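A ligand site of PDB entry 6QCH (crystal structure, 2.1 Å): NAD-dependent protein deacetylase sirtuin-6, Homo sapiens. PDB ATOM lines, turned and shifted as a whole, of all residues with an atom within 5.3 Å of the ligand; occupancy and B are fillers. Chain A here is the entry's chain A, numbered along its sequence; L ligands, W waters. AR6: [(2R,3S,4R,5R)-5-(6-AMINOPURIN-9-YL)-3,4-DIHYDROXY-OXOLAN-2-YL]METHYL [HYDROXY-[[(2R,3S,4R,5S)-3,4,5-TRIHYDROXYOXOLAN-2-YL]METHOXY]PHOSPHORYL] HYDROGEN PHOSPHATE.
O5' of the ligand lies within hydrogen-bond range of N of Ser 210 (3.3 Å).
An oxygen (O1A) of the ligand lies within hydrogen-bond range of the side-chain hydroxyl (OG) of Ser 210.
O3D of the ligand is in hydrogen-bond range of ND1 of His 127 (2.5 Å).
An oxygen (O2') of the ligand lies close to the backbone NH of Gln 236, 3.3 Å away.
O3' of the ligand sits at hydrogen-bond distance from OE1 of Gln 236, at 2.7 Å.
The side-chain hydroxyl (OG1) of Thr 51 sits at hydrogen-bond distance from a nitrogen (N7) of the ligand, at 2.7 Å.
N of Arg 59 lies within hydrogen-bond range of O2A of the ligand.
NH1 of Arg 59 lies within salt-bridge range of O1A of the ligand (2.9 Å).
The side-chain amide nitrogen (ND2) of Asn 234 sits at hydrogen-bond distance from an oxygen (O3') of the ligand, 2.8 Å away.
O2A of the ligand sits at hydrogen-bond distance from N of Phe 58 (2.9 Å).
The backbone NH (N) of Val 252 lies within hydrogen-bond range of a nitrogen (N1) of the ligand.
OG1 of Thr 209 sits at hydrogen-bond distance from O2B of the ligand (2.9 Å).
An oxygen (O1B) of the ligand is in hydrogen-bond range of the backbone NH of Ala 47 (3.0 Å).
O of Gln 107 sits at hydrogen-bond distance from O3D of the ligand, at 3.0 Å.
An oxygen (O1D) of the ligand is in hydrogen-bond range of the indole nitrogen of Trp 65, 3.4 Å away.
N of Leu 235 lies within hydrogen-bond range of N3 of the ligand, 3.4 Å away.
A ring nitrogen (ND1) of His 127 sits at hydrogen-bond distance from the backbone carbonyl oxygen (O) of Gln 107, at 3.2 Å.
O of Arg 59 is in hydrogen-bond range of NE2 of Gln 236, 3.2 Å away.
The backbone carbonyl oxygen (O) of Gly 48 sits at hydrogen-bond distance from the side-chain hydroxyl (OG1) of Thr 51.
The backbone carbonyl oxygen of Phe 58 sits at hydrogen-bond distance from the backbone NH of Trp 65 (2.9 Å).
The side-chain hydroxyl (OG1) of Thr 209 sits at hydrogen-bond distance from the backbone NH (N) of Leu 211.
The backbone NH of Gln 107 lies within hydrogen-bond range of the backbone carbonyl oxygen of Thr 45, at 3.1 Å.
The backbone carbonyl oxygen (O) of Val 233 lies within hydrogen-bond range of the backbone NH (N) of Gly 208 (3.0 Å).
The backbone carbonyl oxygen (O) of Gly 46 is in hydrogen-bond range of the side-chain amide nitrogen (ND2) of Asn 108 (3.2 Å).
O of Gly 48 lies close to N7 of the ligand (3.4 Å).
O of Gly 208 sits close to O4' of the ligand.
CA of Gly 46 touches O1B of the ligand, 3.1 Å away.
Asp 57 touches the ligand.
Trp 182 touches the ligand (CH2 to O1D, 3.7 Å).
CG1 of Ile 213 touches O4D of the ligand, at 3.7 Å.
Gly 250 touches the ligand (O to C2, 3.2 Å).
Tyr 251 touches the ligand.
Hydrophobic or aromatic side chains that line the ligand: Ala 47, Phe 58, Trp 65, His 127, Trp 182, Ile 213, Leu 235, Tyr 251 and Val 252.
Within 4 Å of the ligand: Gly 46, Ala 47, Gly 48, Thr 51, Asp 57, Phe 58, Arg 59, Trp 65, Gln 107, His 127, Trp 182, Gly 208, Thr 209, Ser 210, Ile 213, Asn 234, Leu 235, Gln 236, Gly 250, Tyr 251 and Val 252.
Water W3 lies within hydrogen-bond range of OG of Ser 210, O2B of the ligand, N of Gln 212 and N of Leu 211.
Water W4 lies within hydrogen-bond range of an oxygen (O1B) of the ligand (2.8 Å), the side-chain amide oxygen of Asn 108 (2.9 Å) and the backbone carbonyl oxygen of Gln 107 (3.3 Å).
Water W2 lies within hydrogen-bond range of N of Ala 52 (2.8 Å), O of Gly 48 (3.0 Å), OG1 of Thr 51 (3.2 Å) and N6 of the ligand (3.4 Å).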
ATOM      1  N   GLU A  16      10.058   2.860   7.717  1.00  0.00           N
ATOM      2  CA  GLU A  16       9.804   4.306   7.495  1.00  0.00           C
ATOM      3  C   GLU A  16       9.709   4.564   6.009  1.00  0.00           C
ATOM      4  O   GLU A  16      10.304   3.818   5.237  1.00  0.00           O
ATOM      5  CB  GLU A  16      10.857   5.131   8.221  1.00  0.00           C
ATOM      6  CG  GLU A  16      10.568   5.157   9.679  1.00  0.00           C
ATOM      7  CD  GLU A  16      11.536   6.030  10.462  1.00  0.00           C
ATOM      8  OE1 GLU A  16      12.682   6.175  10.028  1.00  0.00           O
ATOM      9  OE2 GLU A  16      11.095   6.619  11.461  1.00  0.00           O
ATOM     10  N   THR A  45      -2.982  14.844  16.757  1.00  0.00           N
ATOM     11  CA  THR A  45      -1.554  14.571  17.023  1.00  0.00           C
ATOM     12  C   THR A  45      -1.400  13.329  17.853  1.00  0.00           C
ATOM     13  O   THR A  45      -2.323  12.998  18.628  1.00  0.00           O
ATOM     14  CB  THR A  45      -0.858  15.777  17.662  1.00  0.00           C
ATOM     15  OG1 THR A  45      -1.419  16.065  18.936  1.00  0.00           O
ATOM     16  CG2 THR A  45      -0.917  16.972  16.775  1.00  0.00           C
ATOM     17  N   GLY A  46      -0.282  12.634  17.602  1.00  0.00           N
ATOM     18  CA  GLY A  46       0.187  11.459  18.342  1.00  0.00           C
ATOM     19  C   GLY A  46       1.690  11.670  18.632  1.00  0.00           C
ATOM     20  O   GLY A  46       2.200  12.825  18.339  1.00  0.00           O
ATOM     21  N   ALA A  47       2.328  10.603  19.108  1.00  0.00           N
ATOM     22  CA  ALA A  47       3.586  10.563  19.853  1.00  0.00           C
ATOM     23  C   ALA A  47       4.764  11.063  18.978  1.00  0.00           C
ATOM     24  O   ALA A  47       5.699  11.619  19.559  1.00  0.00           O
ATOM     25  CB  ALA A  47       3.716   9.174  20.377  1.00  0.00           C
ATOM     26  N   GLY A  48       4.640  10.957  17.648  1.00  0.00           N
ATOM     27  CA  GLY A  48       5.589  11.339  16.613  1.00  0.00           C
ATOM     28  C   GLY A  48       5.796  12.831  16.580  1.00  0.00           C
ATOM     29  O   GLY A  48       6.899  13.177  16.306  1.00  0.00           O
ATOM     30  N   ILE A  49       4.887  13.669  17.153  1.00  0.00           N
ATOM     31  CA  ILE A  49       5.271  15.115  17.272  1.00  0.00           C
ATOM     32  C   ILE A  49       6.207  15.387  18.453  1.00  0.00           C
ATOM     33  O   ILE A  49       6.485  16.578  18.674  1.00  0.00           O
ATOM     34  CB  ILE A  49       4.060  16.084  17.318  1.00  0.00           C
ATOM     35  CG1 ILE A  49       3.260  16.030  18.623  1.00  0.00           C
ATOM     36  CG2 ILE A  49       3.172  15.929  16.122  1.00  0.00           C
ATOM     37  CD1 ILE A  49       2.384  17.233  18.775  1.00  0.00           C
ATOM     38  N   THR A  51       8.898  13.276  19.399  1.00  0.00           N
ATOM     39  CA  THR A  51      10.147  12.513  19.205  1.00  0.00           C
ATOM     40  C   THR A  51      11.331  13.501  19.096  1.00  0.00           C
ATOM     41  O   THR A  51      12.351  13.192  19.712  1.00  0.00           O
ATOM     42  CB  THR A  51      10.066  11.524  18.060  1.00  0.00           C
ATOM     43  OG1 THR A  51       9.641  12.090  16.832  1.00  0.00           O
ATOM     44  CG2 THR A  51       9.194  10.320  18.429  1.00  0.00           C
ATOM     45  N   ALA A  52      11.148  14.646  18.404  1.00  0.00           N
ATOM     46  CA  ALA A  52      12.194  15.688  18.254  1.00  0.00           C
ATOM     47  C   ALA A  52      12.423  16.427  19.583  1.00  0.00           C
ATOM     48  O   ALA A  52      13.455  17.084  19.684  1.00  0.00           O
ATOM     49  CB  ALA A  52      11.863  16.609  17.089  1.00  0.00           C
ATOM     50  N   ASP A  57       8.432   7.431  20.792  1.00  0.00           N
ATOM     51  CA  ASP A  57       7.051   7.073  20.415  1.00  0.00           C
ATOM     52  C   ASP A  57       6.709   5.642  20.843  1.00  0.00           C
ATOM     53  O   ASP A  57       7.417   5.047  21.589  1.00  0.00           O
ATOM     54  CB  ASP A  57       6.773   7.443  18.955  1.00  0.00           C
ATOM     55  CG  ASP A  57       7.544   6.664  17.939  1.00  0.00           C
ATOM     56  OD1 ASP A  57       8.102   5.681  18.293  1.00  0.00           O
ATOM     57  OD2 ASP A  57       7.531   7.058  16.814  1.00  0.00           O
ATOM     58  N   PHE A  58       5.578   5.117  20.408  1.00  0.00           N
ATOM     59  CA  PHE A  58       5.157   3.769  20.815  1.00  0.00           C
ATOM     60  C   PHE A  58       5.590   2.708  19.772  1.00  0.00           C
ATOM     61  O   PHE A  58       6.014   1.586  20.157  1.00  0.00           O
ATOM     62  CB  PHE A  58       3.669   3.810  21.140  1.00  0.00           C
ATOM     63  CG  PHE A  58       3.412   4.634  22.370  1.00  0.00           C
ATOM     64  CD1 PHE A  58       3.553   4.064  23.626  1.00  0.00           C
ATOM     65  CD2 PHE A  58       2.998   5.964  22.277  1.00  0.00           C
ATOM     66  CE1 PHE A  58       3.412   4.819  24.765  1.00  0.00           C
ATOM     67  CE2 PHE A  58       2.773   6.698  23.446  1.00  0.00           C
ATOM     68  CZ  PHE A  58       2.994   6.128  24.682  1.00  0.00           C
ATOM     69  N   ARG A  59       5.361   2.982  18.509  1.00  0.00           N
ATOM     70  CA  ARG A  59       5.352   1.935  17.481  1.00  0.00           C
ATOM     71  C   ARG A  59       6.345   2.265  16.371  1.00  0.00           C
ATOM     72  O   ARG A  59       6.344   1.491  15.417  1.00  0.00           O
ATOM     73  CB  ARG A  59       3.941   1.761  16.942  1.00  0.00           C
ATOM     74  CG  ARG A  59       2.963   1.482  18.086  1.00  0.00           C
ATOM     75  CD  ARG A  59       1.612   1.148  17.452  1.00  0.00           C
ATOM     76  NE  ARG A  59       0.699   0.805  18.508  1.00  0.00           N
ATOM     77  CZ  ARG A  59       0.230   1.668  19.425  1.00  0.00           C
ATOM     78  NH1 ARG A  59       0.476   2.970  19.331  1.00  0.00           N
ATOM     79  NH2 ARG A  59      -0.623   1.262  20.356  1.00  0.00           N
ATOM     80  N   GLY A  60       7.089   3.359  16.472  1.00  0.00           N
ATOM     81  CA  GLY A  60       8.187   3.703  15.525  1.00  0.00           C
ATOM     82  C   GLY A  60       9.367   2.762  15.735  1.00  0.00           C
ATOM     83  O   GLY A  60       9.372   1.905  16.620  1.00  0.00           O
ATOM     84  N   PRO A  61      10.451   2.883  14.944  1.00  0.00           N
ATOM     85  CA  PRO A  61      11.511   1.894  14.983  1.00  0.00           C
ATOM     86  C   PRO A  61      12.122   1.670  16.369  1.00  0.00           C
ATOM     87  O   PRO A  61      12.529   0.553  16.597  1.00  0.00           O
ATOM     88  CB  PRO A  61      12.566   2.452  14.015  1.00  0.00           C
ATOM     89  CG  PRO A  61      11.758   3.227  13.021  1.00  0.00           C
ATOM     90  CD  PRO A  61      10.573   3.795  13.791  1.00  0.00           C
ATOM     91  N   TRP A  65       6.811   0.199  22.538  1.00  0.00           N
ATOM     92  CA  TRP A  65       6.334  -1.173  22.244  1.00  0.00           C
ATOM     93  C   TRP A  65       7.294  -1.850  21.270  1.00  0.00           C
ATOM     94  O   TRP A  65       7.579  -3.040  21.460  1.00  0.00           O
ATOM     95  CB  TRP A  65       4.914  -1.216  21.665  1.00  0.00           C
ATOM     96  CG  TRP A  65       3.820  -0.504  22.392  1.00  0.00           C
ATOM     97  CD1 TRP A  65       2.681  -0.032  21.811  1.00  0.00           C
ATOM     98  CD2 TRP A  65       3.677  -0.245  23.798  1.00  0.00           C
ATOM     99  NE1 TRP A  65       1.874   0.568  22.742  1.00  0.00           N
ATOM    100  CE2 TRP A  65       2.443   0.423  23.969  1.00  0.00           C
ATOM    101  CE3 TRP A  65       4.470  -0.489  24.923  1.00  0.00           C
ATOM    102  CZ2 TRP A  65       1.996   0.853  25.206  1.00  0.00           C
ATOM    103  CZ3 TRP A  65       4.047  -0.034  26.148  1.00  0.00           C
ATOM    104  CH2 TRP A  65       2.821   0.632  26.289  1.00  0.00           C
ATOM    105  N   GLN A 107      -3.849  12.358  21.283  1.00  0.00           N
ATOM    106  CA  GLN A 107      -3.611  11.105  22.009  1.00  0.00           C
ATOM    107  C   GLN A 107      -2.446  11.242  22.972  1.00  0.00           C
ATOM    108  O   GLN A 107      -2.244  10.289  23.713  1.00  0.00           O
ATOM    109  CB  GLN A 107      -3.324  10.049  20.954  1.00  0.00           C
ATOM    110  CG  GLN A 107      -4.585   9.755  20.164  1.00  0.00           C
ATOM    111  CD  GLN A 107      -4.357   8.807  19.026  1.00  0.00           C
ATOM    112  OE1 GLN A 107      -4.346   7.586  19.182  1.00  0.00           O
ATOM    113  NE2 GLN A 107      -4.216   9.386  17.848  1.00  0.00           N
ATOM    114  N   ASN A 108      -1.683  12.331  22.950  1.00  0.00           N
ATOM    115  CA  ASN A 108      -0.443  12.447  23.803  1.00  0.00           C
ATOM    116  C   ASN A 108      -0.749  12.770  25.232  1.00  0.00           C
ATOM    117  O   ASN A 108      -1.602  13.637  25.497  1.00  0.00           O
ATOM    118  CB  ASN A 108       0.535  13.501  23.298  1.00  0.00           C
ATOM    119  CG  ASN A 108       0.818  13.136  21.869  1.00  0.00           C
ATOM    120  OD1 ASN A 108       0.529  11.992  21.521  1.00  0.00           O
ATOM    121  ND2 ASN A 108       1.321  14.075  21.100  1.00  0.00           N
ATOM    122  N   HIS A 127      -6.283  10.556  25.845  1.00  0.00           N
ATOM    123  CA  HIS A 127      -5.644   9.508  26.676  1.00  0.00           C
ATOM    124  C   HIS A 127      -5.245  10.066  28.034  1.00  0.00           C
ATOM    125  O   HIS A 127      -4.652   9.284  28.808  1.00  0.00           O
ATOM    126  CB  HIS A 127      -4.468   8.799  25.956  1.00  0.00           C
ATOM    127  CG  HIS A 127      -4.921   8.140  24.689  1.00  0.00           C
ATOM    128  ND1 HIS A 127      -4.050   7.662  23.707  1.00  0.00           N
ATOM    129  CD2 HIS A 127      -6.189   7.955  24.235  1.00  0.00           C
ATOM    130  CE1 HIS A 127      -4.744   7.178  22.703  1.00  0.00           C
ATOM    131  NE2 HIS A 127      -6.119   7.414  23.005  1.00  0.00           N
ATOM    132  N   TRP A 182      -5.623   0.446  29.739  1.00  0.00           N
ATOM    133  CA  TRP A 182      -6.123  -0.218  28.504  1.00  0.00           C
ATOM    134  C   TRP A 182      -7.654  -0.428  28.538  1.00  0.00           C
ATOM    135  O   TRP A 182      -8.233  -0.384  27.442  1.00  0.00           O
ATOM    136  CB  TRP A 182      -5.377  -1.540  28.257  1.00  0.00           C
ATOM    137  CG  TRP A 182      -4.019  -1.291  27.684  1.00  0.00           C
ATOM    138  CD1 TRP A 182      -2.841  -1.211  28.361  1.00  0.00           C
ATOM    139  CD2 TRP A 182      -3.711  -0.996  26.308  1.00  0.00           C
ATOM    140  NE1 TRP A 182      -1.816  -0.921  27.506  1.00  0.00           N
ATOM    141  CE2 TRP A 182      -2.317  -0.783  26.232  1.00  0.00           C
ATOM    142  CE3 TRP A 182      -4.469  -0.912  25.132  1.00  0.00           C
ATOM    143  CZ2 TRP A 182      -1.674  -0.491  25.039  1.00  0.00           C
ATOM    144  CZ3 TRP A 182      -3.826  -0.620  23.939  1.00  0.00           C
ATOM    145  CH2 TRP A 182      -2.446  -0.420  23.896  1.00  0.00           C
ATOM    146  N   GLY A 208       2.027  12.607  13.046  1.00  0.00           N
ATOM    147  CA  GLY A 208       2.776  11.811  14.025  1.00  0.00           C
ATOM    148  C   GLY A 208       1.892  10.812  14.752  1.00  0.00           C
ATOM    149  O   GLY A 208       2.252  10.442  15.912  1.00  0.00           O
ATOM    150  N   THR A 209       0.739  10.388  14.182  1.00  0.00           N
ATOM    151  CA  THR A 209      -0.043   9.222  14.696  1.00  0.00           C
ATOM    152  C   THR A 209      -0.150   8.094  13.644  1.00  0.00           C
ATOM    153  O   THR A 209      -0.344   8.396  12.482  1.00  0.00           O
ATOM    154  CB  THR A 209      -1.403   9.643  15.285  1.00  0.00           C
ATOM    155  OG1 THR A 209      -2.090   8.422  15.621  1.00  0.00           O
ATOM    156  CG2 THR A 209      -2.206  10.478  14.347  1.00  0.00           C
ATOM    157  N   SER A 210       0.049   6.829  14.066  1.00  0.00           N
ATOM    158  CA  SER A 210      -0.169   5.602  13.259  1.00  0.00           C
ATOM    159  C   SER A 210      -1.664   5.287  13.156  1.00  0.00           C
ATOM    160  O   SER A 210      -1.968   4.476  12.272  1.00  0.00           O
ATOM    161  CB  SER A 210       0.613   4.359  13.722  1.00  0.00           C
ATOM    162  OG  SER A 210       0.291   3.954  15.058  1.00  0.00           O
ATOM    163  N   LEU A 211      -2.536   5.934  13.934  1.00  0.00           N
ATOM    164  CA  LEU A 211      -4.023   5.877  13.792  1.00  0.00           C
ATOM    165  C   LEU A 211      -4.582   4.472  14.140  1.00  0.00           C
ATOM    166  O   LEU A 211      -5.654   4.096  13.649  1.00  0.00           O
ATOM    167  CB  LEU A 211      -4.372   6.324  12.369  1.00  0.00           C
ATOM    168  CG  LEU A 211      -4.122   7.808  12.040  1.00  0.00           C
ATOM    169  CD1 LEU A 211      -4.438   8.121  10.598  1.00  0.00           C
ATOM    170  CD2 LEU A 211      -4.873   8.752  12.959  1.00  0.00           C
ATOM    171  N   GLN A 212      -4.005   3.770  15.104  1.00  0.00           N
ATOM    172  CA  GLN A 212      -4.257   2.315  15.264  1.00  0.00           C
ATOM    173  C   GLN A 212      -5.192   2.100  16.445  1.00  0.00           C
ATOM    174  O   GLN A 212      -5.509   0.955  16.737  1.00  0.00           O
ATOM    175  CB  GLN A 212      -2.916   1.581  15.425  1.00  0.00           C
ATOM    176  CG  GLN A 212      -2.234   1.217  14.103  1.00  0.00           C
ATOM    177  CD  GLN A 212      -1.006   0.409  14.426  1.00  0.00           C
ATOM    178  OE1 GLN A 212      -1.128  -0.705  14.885  1.00  0.00           O
ATOM    179  NE2 GLN A 212       0.191   0.941  14.204  1.00  0.00           N
ATOM    180  N   ILE A 213      -5.480   3.160  17.199  1.00  0.00           N
ATOM    181  CA  ILE A 213      -6.281   3.084  18.450  1.00  0.00           C
ATOM    182  C   ILE A 213      -7.673   3.625  18.121  1.00  0.00           C
ATOM    183  O   ILE A 213      -7.793   4.709  17.534  1.00  0.00           O
ATOM    184  CB  ILE A 213      -5.597   3.859  19.584  1.00  0.00           C
ATOM    185  CG1 ILE A 213      -4.184   3.325  19.825  1.00  0.00           C
ATOM    186  CG2 ILE A 213      -6.436   3.829  20.853  1.00  0.00           C
ATOM    187  CD1 ILE A 213      -4.148   2.032  20.607  1.00  0.00           C
ATOM    188  N   VAL A 233       0.201  13.119   7.930  1.00  0.00           N
ATOM    189  CA  VAL A 233       1.679  13.349   7.911  1.00  0.00           C
ATOM    190  C   VAL A 233       2.288  12.302   8.851  1.00  0.00           C
ATOM    191  O   VAL A 233       1.974  12.275  10.060  1.00  0.00           O
ATOM    192  CB  VAL A 233       2.069  14.795   8.293  1.00  0.00           C
ATOM    193  CG1 VAL A 233       3.581  15.052   8.261  1.00  0.00           C
ATOM    194  CG2 VAL A 233       1.411  15.853   7.398  1.00  0.00           C
ATOM    195  N   ASN A 234       3.115  11.422   8.304  1.00  0.00           N
ATOM    196  CA  ASN A 234       3.689  10.311   9.092  1.00  0.00           C
ATOM    197  C   ASN A 234       4.843   9.622   8.393  1.00  0.00           C
ATOM    198  O   ASN A 234       4.713   9.301   7.210  1.00  0.00           O
ATOM    199  CB  ASN A 234       2.656   9.234   9.404  1.00  0.00           C
ATOM    200  CG  ASN A 234       2.920   8.599  10.746  1.00  0.00           C
ATOM    201  OD1 ASN A 234       2.986   9.278  11.767  1.00  0.00           O
ATOM    202  ND2 ASN A 234       2.992   7.267  10.793  1.00  0.00           N
ATOM    203  N   LEU A 235       5.890   9.301   9.159  1.00  0.00           N
ATOM    204  CA  LEU A 235       7.039   8.538   8.672  1.00  0.00           C
ATOM    205  C   LEU A 235       6.667   7.052   8.294  1.00  0.00           C
ATOM    206  O   LEU A 235       6.978   6.606   7.190  1.00  0.00           O
ATOM    207  CB  LEU A 235       8.099   8.649   9.768  1.00  0.00           C
ATOM    208  CG  LEU A 235       8.937   9.924   9.714  1.00  0.00           C
ATOM    209  CD1 LEU A 235      10.018   9.921  10.796  1.00  0.00           C
ATOM    210  CD2 LEU A 235       9.502  10.135   8.302  1.00  0.00           C
ATOM    211  N   GLN A 236       5.961   6.307   9.128  1.00  0.00           N
ATOM    212  CA  GLN A 236       5.479   4.945   8.804  1.00  0.00           C
ATOM    213  C   GLN A 236       4.120   5.009   8.112  1.00  0.00           C
ATOM    214  O   GLN A 236       3.464   6.027   8.175  1.00  0.00           O
ATOM    215  CB  GLN A 236       5.287   4.143  10.068  1.00  0.00           C
ATOM    216  CG  GLN A 236       6.578   3.917  10.795  1.00  0.00           C
ATOM    217  CD  GLN A 236       6.336   3.251  12.122  1.00  0.00           C
ATOM    218  OE1 GLN A 236       5.329   3.481  12.813  1.00  0.00           O
ATOM    219  NE2 GLN A 236       7.286   2.413  12.477  1.00  0.00           N
ATOM    220  N   PRO A 237       3.676   3.894   7.506  1.00  0.00           N
ATOM    221  CA  PRO A 237       2.286   3.726   7.094  1.00  0.00           C
ATOM    222  C   PRO A 237       1.384   4.002   8.301  1.00  0.00           C
ATOM    223  O   PRO A 237       1.884   3.974   9.365  1.00  0.00           O
ATOM    224  CB  PRO A 237       2.214   2.241   6.644  1.00  0.00           C
ATOM    225  CG  PRO A 237       3.638   1.908   6.245  1.00  0.00           C
ATOM    226  CD  PRO A 237       4.498   2.690   7.214  1.00  0.00           C
ATOM    227  N   GLY A 250       7.494  12.420   5.927  1.00  0.00           N
ATOM    228  CA  GLY A 250       8.558  13.344   6.344  1.00  0.00           C
ATOM    229  C   GLY A 250       8.463  13.609   7.831  1.00  0.00           C
ATOM    230  O   GLY A 250       7.466  13.176   8.498  1.00  0.00           O
ATOM    231  N   TYR A 251       9.526  14.172   8.374  1.00  0.00           N
ATOM    232  CA  TYR A 251       9.603  14.661   9.758  1.00  0.00           C
ATOM    233  C   TYR A 251       8.580  15.768   9.899  1.00  0.00           C
ATOM    234  O   TYR A 251       8.634  16.656   9.048  1.00  0.00           O
ATOM    235  CB  TYR A 251      11.004  15.182  10.024  1.00  0.00           C
ATOM    236  CG  TYR A 251      12.000  14.065  10.008  1.00  0.00           C
ATOM    237  CD1 TYR A 251      12.000  13.144  11.025  1.00  0.00           C
ATOM    238  CD2 TYR A 251      12.860  13.871   8.935  1.00  0.00           C
ATOM    239  CE1 TYR A 251      12.884  12.095  11.036  1.00  0.00           C
ATOM    240  CE2 TYR A 251      13.775  12.821   8.951  1.00  0.00           C
ATOM    241  CZ  TYR A 251      13.781  11.944  10.011  1.00  0.00           C
ATOM    242  OH  TYR A 251      14.650  10.901  10.094  1.00  0.00           O
ATOM    243  N   VAL A 252       7.731  15.726  10.934  1.00  0.00           N
ATOM    244  CA  VAL A 252       6.668  16.744  11.120  1.00  0.00           C
ATOM    245  C   VAL A 252       7.278  18.146  11.278  1.00  0.00           C
ATOM    246  O   VAL A 252       6.796  19.063  10.641  1.00  0.00           O
ATOM    247  CB  VAL A 252       5.679  16.341  12.225  1.00  0.00           C
ATOM    248  CG1 VAL A 252       4.854  15.153  11.758  1.00  0.00           C
ATOM    249  CG2 VAL A 252       6.372  16.041  13.573  1.00  0.00           C
ATOM    250  N   ASP A 253       8.417  18.268  11.944  1.00  0.00           N
ATOM    251  CA  ASP A 253       9.041  19.601  12.112  1.00  0.00           C
ATOM    252  C   ASP A 253       9.371  20.215  10.751  1.00  0.00           C
ATOM    253  O   ASP A 253       9.154  21.403  10.607  1.00  0.00           O
ATOM    254  CB  ASP A 253      10.256  19.563  13.047  1.00  0.00           C
ATOM    255  CG  ASP A 253       9.761  19.635  14.462  1.00  0.00           C
ATOM    256  OD1 ASP A 253       8.497  19.827  14.655  1.00  0.00           O
ATOM    257  OD2 ASP A 253      10.606  19.530  15.348  1.00  0.00           O
HETATM  258  N1  AR6 L   1       7.971  13.062  12.096  1.00  0.00           N
HETATM  259  C2  AR6 L   1       6.974  12.319  11.568  1.00  0.00           C
HETATM  260  N3  AR6 L   1       6.535  11.118  11.963  1.00  0.00           N
HETATM  261  C4  AR6 L   1       7.102  10.722  13.105  1.00  0.00           C
HETATM  262  C5  AR6 L   1       8.153  11.346  13.746  1.00  0.00           C
HETATM  263  C6  AR6 L   1       8.602  12.589  13.216  1.00  0.00           C
HETATM  264  N6  AR6 L   1       9.554  13.362  13.764  1.00  0.00           N
HETATM  265  N7  AR6 L   1       8.501  10.581  14.858  1.00  0.00           N
HETATM  266  C8  AR6 L   1       7.649   9.585  14.894  1.00  0.00           C
HETATM  267  N9  AR6 L   1       6.849   9.553  13.782  1.00  0.00           N
HETATM  268  PA  AR6 L   1       2.477   5.610  17.537  1.00  0.00           P
HETATM  269  PB  AR6 L   1       0.214   7.129  18.725  1.00  0.00           P
HETATM  270  C1' AR6 L   1       5.770   8.545  13.471  1.00  0.00           C
HETATM  271  O1A AR6 L   1       1.530   4.508  17.137  1.00  0.00           O
HETATM  272  O1B AR6 L   1       0.194   8.508  19.284  1.00  0.00           O
HETATM  273  C1D AR6 L   1      -0.362   4.012  22.929  1.00  0.00           C
HETATM  274  O1D AR6 L   1      -0.651   2.747  23.379  1.00  0.00           O
HETATM  275  C2' AR6 L   1       6.065   7.070  13.637  1.00  0.00           C
HETATM  276  O2' AR6 L   1       6.489   6.558  12.420  1.00  0.00           O
HETATM  277  O2A AR6 L   1       3.827   5.268  18.113  1.00  0.00           O
HETATM  278  O2B AR6 L   1      -0.440   6.810  17.415  1.00  0.00           O
HETATM  279  C2D AR6 L   1      -0.733   5.203  23.813  1.00  0.00           C
HETATM  280  O2D AR6 L   1      -2.009   5.135  24.424  1.00  0.00           O
HETATM  281  C3' AR6 L   1       4.701   6.443  14.057  1.00  0.00           C
HETATM  282  O3' AR6 L   1       4.055   5.819  12.964  1.00  0.00           O
HETATM  283  O3A AR6 L   1       1.765   6.589  18.599  1.00  0.00           O
HETATM  284  C3D AR6 L   1      -0.811   6.306  22.761  1.00  0.00           C
HETATM  285  O3D AR6 L   1      -1.615   7.409  23.137  1.00  0.00           O
HETATM  286  C4' AR6 L   1       3.904   7.646  14.584  1.00  0.00           C
HETATM  287  O4' AR6 L   1       4.754   8.791  14.404  1.00  0.00           O
HETATM  288  C4D AR6 L   1      -1.601   5.574  21.672  1.00  0.00           C
HETATM  289  O4D AR6 L   1      -1.145   4.220  21.737  1.00  0.00           O
HETATM  290  C5' AR6 L   1       3.422   7.650  16.008  1.00  0.00           C
HETATM  291  O5' AR6 L   1       2.557   6.502  16.239  1.00  0.00           O
HETATM  292  C5D AR6 L   1      -1.534   6.040  20.251  1.00  0.00           C
HETATM  293  O5D AR6 L   1      -0.161   6.082  19.852  1.00  0.00           O
HETATM  294  O   HOH W   1      -3.709   5.880  17.130  1.00  0.00           O
HETATM  295  O   HOH W   2       9.074  15.237  16.576  1.00  0.00           O
HETATM  296  O   HOH W   3      -1.529   4.524  16.640  1.00  0.00           O
HETATM  297  O   HOH W   4       0.271   9.148  21.971  1.00  0.00           O
HETATM  298  O   HOH W   5       9.580  16.303  13.632  1.00  0.00           O
